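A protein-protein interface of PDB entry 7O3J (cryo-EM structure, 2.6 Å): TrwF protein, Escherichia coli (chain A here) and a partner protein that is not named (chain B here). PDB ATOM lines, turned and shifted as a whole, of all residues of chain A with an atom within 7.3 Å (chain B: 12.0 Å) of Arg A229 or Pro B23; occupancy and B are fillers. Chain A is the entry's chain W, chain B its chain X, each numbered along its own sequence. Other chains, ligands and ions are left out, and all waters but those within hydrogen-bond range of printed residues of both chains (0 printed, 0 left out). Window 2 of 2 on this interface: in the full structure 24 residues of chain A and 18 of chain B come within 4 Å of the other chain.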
ATOM      1  N   ILE A 168      21.398  30.372 -18.227  1.00  0.00           N
ATOM      2  CA  ILE A 168      21.956  29.073 -18.563  1.00  0.00           C
ATOM      3  C   ILE A 168      23.440  29.180 -18.918  1.00  0.00           C
ATOM      4  O   ILE A 168      23.990  28.280 -19.543  1.00  0.00           O
ATOM      5  CB  ILE A 168      21.168  28.393 -19.691  1.00  0.00           C
ATOM      6  CG1 ILE A 168      21.237  29.221 -20.972  1.00  0.00           C
ATOM      7  CG2 ILE A 168      19.732  28.186 -19.283  1.00  0.00           C
ATOM      8  CD1 ILE A 168      20.862  28.451 -22.197  1.00  0.00           C
ATOM      9  N   LEU A 190      22.790  21.179 -16.746  1.00  0.00           N
ATOM     10  CA  LEU A 190      23.700  21.111 -17.878  1.00  0.00           C
ATOM     11  C   LEU A 190      22.916  21.278 -19.171  1.00  0.00           C
ATOM     12  O   LEU A 190      22.012  20.484 -19.440  1.00  0.00           O
ATOM     13  CB  LEU A 190      24.469  19.804 -17.899  1.00  0.00           C
ATOM     14  CG  LEU A 190      25.536  19.629 -16.830  1.00  0.00           C
ATOM     15  CD1 LEU A 190      26.243  18.318 -17.047  1.00  0.00           C
ATOM     16  CD2 LEU A 190      26.515  20.776 -16.847  1.00  0.00           C
ATOM     17  N   PRO A 191      23.222  22.275 -19.982  1.00  0.00           N
ATOM     18  CA  PRO A 191      22.464  22.500 -21.213  1.00  0.00           C
ATOM     19  C   PRO A 191      22.973  21.676 -22.380  1.00  0.00           C
ATOM     20  O   PRO A 191      23.834  20.810 -22.221  1.00  0.00           O
ATOM     21  CB  PRO A 191      22.667  23.992 -21.458  1.00  0.00           C
ATOM     22  CG  PRO A 191      24.012  24.247 -20.919  1.00  0.00           C
ATOM     23  CD  PRO A 191      24.241  23.310 -19.776  1.00  0.00           C
ATOM     24  N   SER A 192      22.436  21.940 -23.562  1.00  0.00           N
ATOM     25  CA  SER A 192      22.893  21.327 -24.797  1.00  0.00           C
ATOM     26  C   SER A 192      23.698  22.358 -25.575  1.00  0.00           C
ATOM     27  O   SER A 192      23.304  23.523 -25.654  1.00  0.00           O
ATOM     28  CB  SER A 192      21.706  20.827 -25.614  1.00  0.00           C
ATOM     29  OG  SER A 192      22.130  20.018 -26.686  1.00  0.00           O
ATOM     30  N   ILE A 193      24.829  21.938 -26.133  1.00  0.00           N
ATOM     31  CA  ILE A 193      25.775  22.838 -26.782  1.00  0.00           C
ATOM     32  C   ILE A 193      25.872  22.461 -28.251  1.00  0.00           C
ATOM     33  O   ILE A 193      25.977  21.278 -28.583  1.00  0.00           O
ATOM     34  CB  ILE A 193      27.155  22.792 -26.105  1.00  0.00           C
ATOM     35  CG1 ILE A 193      27.023  23.223 -24.650  1.00  0.00           C
ATOM     36  CG2 ILE A 193      28.131  23.690 -26.818  1.00  0.00           C
ATOM     37  CD1 ILE A 193      28.227  22.957 -23.829  1.00  0.00           C
ATOM     38  N   TYR A 194      25.831  23.465 -29.125  1.00  0.00           N
ATOM     39  CA  TYR A 194      25.761  23.248 -30.561  1.00  0.00           C
ATOM     40  C   TYR A 194      26.850  24.020 -31.280  1.00  0.00           C
ATOM     41  O   TYR A 194      27.300  25.072 -30.830  1.00  0.00           O
ATOM     42  CB  TYR A 194      24.397  23.644 -31.116  1.00  0.00           C
ATOM     43  CG  TYR A 194      23.321  22.759 -30.584  1.00  0.00           C
ATOM     44  CD1 TYR A 194      23.142  21.492 -31.092  1.00  0.00           C
ATOM     45  CD2 TYR A 194      22.515  23.168 -29.541  1.00  0.00           C
ATOM     46  CE1 TYR A 194      22.188  20.668 -30.596  1.00  0.00           C
ATOM     47  CE2 TYR A 194      21.554  22.344 -29.041  1.00  0.00           C
ATOM     48  CZ  TYR A 194      21.398  21.094 -29.572  1.00  0.00           C
ATOM     49  OH  TYR A 194      20.435  20.254 -29.085  1.00  0.00           O
ATOM     50  N   GLU A 202      23.303  25.486 -37.100  1.00  0.00           N
ATOM     51  CA  GLU A 202      23.720  24.739 -35.929  1.00  0.00           C
ATOM     52  C   GLU A 202      23.889  23.272 -36.293  1.00  0.00           C
ATOM     53  O   GLU A 202      23.168  22.742 -37.138  1.00  0.00           O
ATOM     54  CB  GLU A 202      22.676  24.876 -34.832  1.00  0.00           C
ATOM     55  CG  GLU A 202      22.547  26.266 -34.281  1.00  0.00           C
ATOM     56  CD  GLU A 202      21.485  26.347 -33.218  1.00  0.00           C
ATOM     57  OE1 GLU A 202      20.781  25.340 -33.013  1.00  0.00           O
ATOM     58  OE2 GLU A 202      21.305  27.429 -32.636  1.00  0.00           O
ATOM     59  N   MET A 227      26.649  27.654 -29.595  1.00  0.00           N
ATOM     60  CA  MET A 227      25.267  27.906 -29.219  1.00  0.00           C
ATOM     61  C   MET A 227      24.901  27.019 -28.043  1.00  0.00           C
ATOM     62  O   MET A 227      25.145  25.813 -28.078  1.00  0.00           O
ATOM     63  CB  MET A 227      24.321  27.637 -30.382  1.00  0.00           C
ATOM     64  CG  MET A 227      22.888  28.001 -30.105  1.00  0.00           C
ATOM     65  SD  MET A 227      22.729  29.700 -29.564  1.00  0.00           S
ATOM     66  CE  MET A 227      22.711  30.513 -31.148  1.00  0.00           C
ATOM     67  N   ILE A 228      24.309  27.611 -27.015  1.00  0.00           N
ATOM     68  CA  ILE A 228      23.916  26.894 -25.811  1.00  0.00           C
ATOM     69  C   ILE A 228      22.407  27.010 -25.670  1.00  0.00           C
ATOM     70  O   ILE A 228      21.865  28.119 -25.653  1.00  0.00           O
ATOM     71  CB  ILE A 228      24.633  27.442 -24.572  1.00  0.00           C
ATOM     72  CG1 ILE A 228      26.134  27.196 -24.686  1.00  0.00           C
ATOM     73  CG2 ILE A 228      24.095  26.801 -23.337  1.00  0.00           C
ATOM     74  CD1 ILE A 228      26.882  27.413 -23.412  1.00  0.00           C
ATOM     75  N   ARG A 229      21.728  25.873 -25.576  1.00  0.00           N
ATOM     76  CA  ARG A 229      20.276  25.832 -25.519  1.00  0.00           C
ATOM     77  C   ARG A 229      19.827  24.947 -24.370  1.00  0.00           C
ATOM     78  O   ARG A 229      20.360  23.852 -24.184  1.00  0.00           O
ATOM     79  CB  ARG A 229      19.686  25.305 -26.822  1.00  0.00           C
ATOM     80  CG  ARG A 229      20.032  26.119 -28.034  1.00  0.00           C
ATOM     81  CD  ARG A 229      19.173  25.725 -29.203  1.00  0.00           C
ATOM     82  NE  ARG A 229      19.369  26.616 -30.335  1.00  0.00           N
ATOM     83  CZ  ARG A 229      18.755  27.780 -30.477  1.00  0.00           C
ATOM     84  NH1 ARG A 229      17.904  28.194 -29.555  1.00  0.00           N
ATOM     85  NH2 ARG A 229      18.993  28.531 -31.538  1.00  0.00           N
ATOM     86  N   LEU A 230      18.846  25.416 -23.611  1.00  0.00           N
ATOM     87  CA  LEU A 230      18.200  24.603 -22.584  1.00  0.00           C
ATOM     88  C   LEU A 230      16.729  24.978 -22.564  1.00  0.00           C
ATOM     89  O   LEU A 230      16.370  26.049 -22.076  1.00  0.00           O
ATOM     90  CB  LEU A 230      18.835  24.817 -21.213  1.00  0.00           C
ATOM     91  CG  LEU A 230      18.261  23.970 -20.081  1.00  0.00           C
ATOM     92  CD1 LEU A 230      18.146  22.523 -20.490  1.00  0.00           C
ATOM     93  CD2 LEU A 230      19.119  24.099 -18.858  1.00  0.00           C
ATOM     94  N   GLY A 231      15.885  24.099 -23.084  1.00  0.00           N
ATOM     95  CA  GLY A 231      14.477  24.407 -23.182  1.00  0.00           C
ATOM     96  C   GLY A 231      14.213  25.458 -24.233  1.00  0.00           C
ATOM     97  O   GLY A 231      14.479  25.239 -25.416  1.00  0.00           O
ATOM     98  N   ASN A 232      13.698  26.609 -23.818  1.00  0.00           N
ATOM     99  CA  ASN A 232      13.413  27.706 -24.730  1.00  0.00           C
ATOM    100  C   ASN A 232      14.296  28.909 -24.433  1.00  0.00           C
ATOM    101  O   ASN A 232      13.895  30.053 -24.633  1.00  0.00           O
ATOM    102  CB  ASN A 232      11.937  28.086 -24.672  1.00  0.00           C
ATOM    103  CG  ASN A 232      11.490  28.865 -25.887  1.00  0.00           C
ATOM    104  OD1 ASN A 232      11.380  28.318 -26.981  1.00  0.00           O
ATOM    105  ND2 ASN A 232      11.229  30.152 -25.701  1.00  0.00           N
ATOM    106  N   ARG A 233      15.501  28.659 -23.942  1.00  0.00           N
ATOM    107  CA  ARG A 233      16.477  29.697 -23.662  1.00  0.00           C
ATOM    108  C   ARG A 233      17.731  29.409 -24.467  1.00  0.00           C
ATOM    109  O   ARG A 233      18.154  28.257 -24.574  1.00  0.00           O
ATOM    110  CB  ARG A 233      16.801  29.751 -22.177  1.00  0.00           C
ATOM    111  CG  ARG A 233      15.597  29.488 -21.315  1.00  0.00           C
ATOM    112  CD  ARG A 233      15.704  30.143 -19.962  1.00  0.00           C
ATOM    113  NE  ARG A 233      16.025  31.564 -20.023  1.00  0.00           N
ATOM    114  CZ  ARG A 233      15.188  32.507 -20.441  1.00  0.00           C
ATOM    115  NH1 ARG A 233      15.571  33.771 -20.448  1.00  0.00           N
ATOM    116  NH2 ARG A 233      13.976  32.189 -20.859  1.00  0.00           N
ATOM    117  N   ALA A 234      18.315  30.450 -25.042  1.00  0.00           N
ATOM    118  CA  ALA A 234      19.483  30.299 -25.892  1.00  0.00           C
ATOM    119  C   ALA A 234      20.545  31.301 -25.481  1.00  0.00           C
ATOM    120  O   ALA A 234      20.232  32.405 -25.037  1.00  0.00           O
ATOM    121  CB  ALA A 234      19.126  30.482 -27.360  1.00  0.00           C
ATOM    122  N   LEU A 235      21.800  30.902 -25.635  1.00  0.00           N
ATOM    123  CA  LEU A 235      22.940  31.739 -25.305  1.00  0.00           C
ATOM    124  C   LEU A 235      24.033  31.480 -26.325  1.00  0.00           C
ATOM    125  O   LEU A 235      24.340  30.323 -26.621  1.00  0.00           O
ATOM    126  CB  LEU A 235      23.442  31.442 -23.894  1.00  0.00           C
ATOM    127  CG  LEU A 235      24.686  32.174 -23.413  1.00  0.00           C
ATOM    128  CD1 LEU A 235      24.324  33.493 -22.805  1.00  0.00           C
ATOM    129  CD2 LEU A 235      25.401  31.321 -22.417  1.00  0.00           C
ATOM    130  N   SER B  19       5.570  26.773 -42.131  1.00  0.00           N
ATOM    131  CA  SER B  19       6.837  26.078 -41.989  1.00  0.00           C
ATOM    132  C   SER B  19       7.152  25.872 -40.515  1.00  0.00           C
ATOM    133  O   SER B  19       6.588  26.534 -39.639  1.00  0.00           O
ATOM    134  CB  SER B  19       7.972  26.850 -42.665  1.00  0.00           C
ATOM    135  OG  SER B  19       9.220  26.229 -42.424  1.00  0.00           O
ATOM    136  N   ALA B  20       8.054  24.940 -40.250  1.00  0.00           N
ATOM    137  CA  ALA B  20       8.413  24.619 -38.876  1.00  0.00           C
ATOM    138  C   ALA B  20       9.100  25.810 -38.223  1.00  0.00           C
ATOM    139  O   ALA B  20      10.041  26.366 -38.799  1.00  0.00           O
ATOM    140  CB  ALA B  20       9.323  23.400 -38.840  1.00  0.00           C
ATOM    141  N   PRO B  21       8.666  26.234 -37.042  1.00  0.00           N
ATOM    142  CA  PRO B  21       9.295  27.392 -36.402  1.00  0.00           C
ATOM    143  C   PRO B  21      10.736  27.106 -36.020  1.00  0.00           C
ATOM    144  O   PRO B  21      11.099  25.980 -35.681  1.00  0.00           O
ATOM    145  CB  PRO B  21       8.425  27.629 -35.165  1.00  0.00           C
ATOM    146  CG  PRO B  21       7.792  26.327 -34.899  1.00  0.00           C
ATOM    147  CD  PRO B  21       7.573  25.683 -36.229  1.00  0.00           C
ATOM    148  N   LYS B  22      11.553  28.137 -36.090  1.00  0.00           N
ATOM    149  CA  LYS B  22      12.951  28.048 -35.718  1.00  0.00           C
ATOM    150  C   LYS B  22      13.104  28.161 -34.205  1.00  0.00           C
ATOM    151  O   LYS B  22      12.251  28.743 -33.532  1.00  0.00           O
ATOM    152  CB  LYS B  22      13.745  29.157 -36.392  1.00  0.00           C
ATOM    153  CG  LYS B  22      13.701  29.129 -37.900  1.00  0.00           C
ATOM    154  CD  LYS B  22      14.466  27.945 -38.449  1.00  0.00           C
ATOM    155  CE  LYS B  22      15.960  28.138 -38.281  1.00  0.00           C
ATOM    156  NZ  LYS B  22      16.728  27.049 -38.934  1.00  0.00           N
ATOM    157  N   PRO B  23      14.175  27.610 -33.646  1.00  0.00           N
ATOM    158  CA  PRO B  23      14.464  27.852 -32.233  1.00  0.00           C
ATOM    159  C   PRO B  23      14.845  29.304 -32.008  1.00  0.00           C
ATOM    160  O   PRO B  23      15.274  30.011 -32.921  1.00  0.00           O
ATOM    161  CB  PRO B  23      15.642  26.917 -31.940  1.00  0.00           C
ATOM    162  CG  PRO B  23      15.674  25.964 -33.064  1.00  0.00           C
ATOM    163  CD  PRO B  23      15.144  26.688 -34.248  1.00  0.00           C
ATOM    164  N   LYS B  24      14.670  29.748 -30.768  1.00  0.00           N
ATOM    165  CA  LYS B  24      14.926  31.142 -30.438  1.00  0.00           C
ATOM    166  C   LYS B  24      16.367  31.519 -30.748  1.00  0.00           C
ATOM    167  O   LYS B  24      17.302  30.800 -30.390  1.00  0.00           O
ATOM    168  CB  LYS B  24      14.626  31.400 -28.963  1.00  0.00           C
ATOM    169  CG  LYS B  24      15.309  32.637 -28.421  1.00  0.00           C
ATOM    170  CD  LYS B  24      15.340  32.651 -26.912  1.00  0.00           C
ATOM    171  CE  LYS B  24      13.944  32.744 -26.348  1.00  0.00           C
ATOM    172  NZ  LYS B  24      13.966  33.166 -24.922  1.00  0.00           N
ATOM    173  N   GLN B  25      16.538  32.637 -31.417  1.00  0.00           N
ATOM    174  CA  GLN B  25      17.854  33.217 -31.647  1.00  0.00           C
ATOM    175  C   GLN B  25      18.204  34.156 -30.503  1.00  0.00           C
ATOM    176  O   GLN B  25      17.418  35.056 -30.191  1.00  0.00           O
ATOM    177  CB  GLN B  25      17.887  33.980 -32.960  1.00  0.00           C
ATOM    178  CG  GLN B  25      18.102  33.117 -34.183  1.00  0.00           C
ATOM    179  CD  GLN B  25      19.438  32.403 -34.164  1.00  0.00           C
ATOM    180  OE1 GLN B  25      19.505  31.183 -34.292  1.00  0.00           O
ATOM    181  NE2 GLN B  25      20.511  33.166 -34.001  1.00  0.00           N
ATOM    182  N   PRO B  26      19.345  33.974 -29.848  1.00  0.00           N
ATOM    183  CA  PRO B  26      19.709  34.869 -28.749  1.00  0.00           C
ATOM    184  C   PRO B  26      19.969  36.286 -29.233  1.00  0.00           C
ATOM    185  O   PRO B  26      20.445  36.512 -30.347  1.00  0.00           O
ATOM    186  CB  PRO B  26      20.982  34.236 -28.186  1.00  0.00           C
ATOM    187  CG  PRO B  26      21.533  33.455 -29.304  1.00  0.00           C
ATOM    188  CD  PRO B  26      20.368  32.946 -30.078  1.00  0.00           C
ATOM    189  N   SER B  27      19.645  37.246 -28.371  1.00  0.00           N
ATOM    190  CA  SER B  27      19.876  38.650 -28.672  1.00  0.00           C
ATOM    191  C   SER B  27      21.362  38.959 -28.578  1.00  0.00           C
ATOM    192  O   SER B  27      22.051  38.452 -27.690  1.00  0.00           O
ATOM    193  CB  SER B  27      19.091  39.537 -27.709  1.00  0.00           C
ATOM    194  OG  SER B  27      19.627  39.458 -26.401  1.00  0.00           O
ATOM    195  N   ASP B  28      21.853  39.799 -29.486  1.00  0.00           N
ATOM    196  CA  ASP B  28      23.274  40.113 -29.564  1.00  0.00           C
ATOM    197  C   ASP B  28      23.621  41.451 -28.925  1.00  0.00           C
ATOM    198  O   ASP B  28      24.509  42.156 -29.416  1.00  0.00           O
ATOM    199  CB  ASP B  28      23.738  40.080 -31.020  1.00  0.00           C
ATOM    200  CG  ASP B  28      25.143  39.538 -31.170  1.00  0.00           C
ATOM    201  OD1 ASP B  28      25.991  39.826 -30.301  1.00  0.00           O
ATOM    202  OD2 ASP B  28      25.402  38.818 -32.156  1.00  0.00           O
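The guanidinium group of Arg A229 sits at hydrogen-bond distance from the backbone carbonyl oxygen of Lys B24 (2.8 Å).
NZ of Lys B24 sits at hydrogen-bond distance from O of Asn A232 (3.1 Å).
O of Ser A192 sits at hydrogen-bond distance from N of Arg A229, 2.8 Å away.
The backbone NH (N) of Tyr A194 is in hydrogen-bond range of the backbone carbonyl oxygen (O) of Met A227 (2.7 Å).
The guanidinium group (NH2) of Arg A229 is in salt-bridge range of the side-chain carboxylate (OE2) of Glu A202.
CD of Pro B26 touches CE of Met A227 (3.5 Å).
Arg A229 touches Pro B23 (NH1 to CB, 3.5 Å).
Arg A229 touches Gln B25.
Lys B24 touches Ala A234.
Pro B26 touches Ala A234.
No residue of chain B comes within 4 Å of Pro A191.
No residue of chain B comes within 4 Å of Ile A193.
Tyr A194 touches none of the printed residues of chain B.
Of chain B, only Pro B26 (3.5 Å) comes within 4 Å of Met A227.
No residue of chain B comes within 4 Å of Ile A228.
Arg A229 touches just these residues of chain B: Pro B23 (3.5 Å), Lys B24 (2.8 Å) and Gln B25 (3.9 Å).
No residue of chain B comes within 4 Å of Leu A230.
Of the printed residues of chain B, Asn A232 touches Lys B24.
Of chain B, only Lys B24 and Pro B26 come within 4 Å of Ala A234.
Printed residues of chain A within 4 Å of Lys B24: Arg A229 (2.8 Å), Asn A232 (3.1 Å) and Ala A234 (3.6 Å).
Of the printed residues of chain A, Gln B25 touches Arg A229.
Printed residues of chain A within 4 Å of Pro B26: Met A227 (3.5 Å) and Ala A234 (3.7 Å).
The nearest residue of chain A that does not touch Pro B23 is Glu A202 (5.1 Å).
Of the 10 printed residues of chain B, 4 touch a printed residue of chain A.
Hydrophobic or aromatic side chains of chain B within 4 Å of the printed part of chain A: Pro B23 and Pro B26.
Among the printed residues, 7 pairs touch across the chains.
Among the printed residues, no Asp or Glu carboxylate lies within 4 Å of a Lys or Arg side-chain nitrogen of the other chain.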
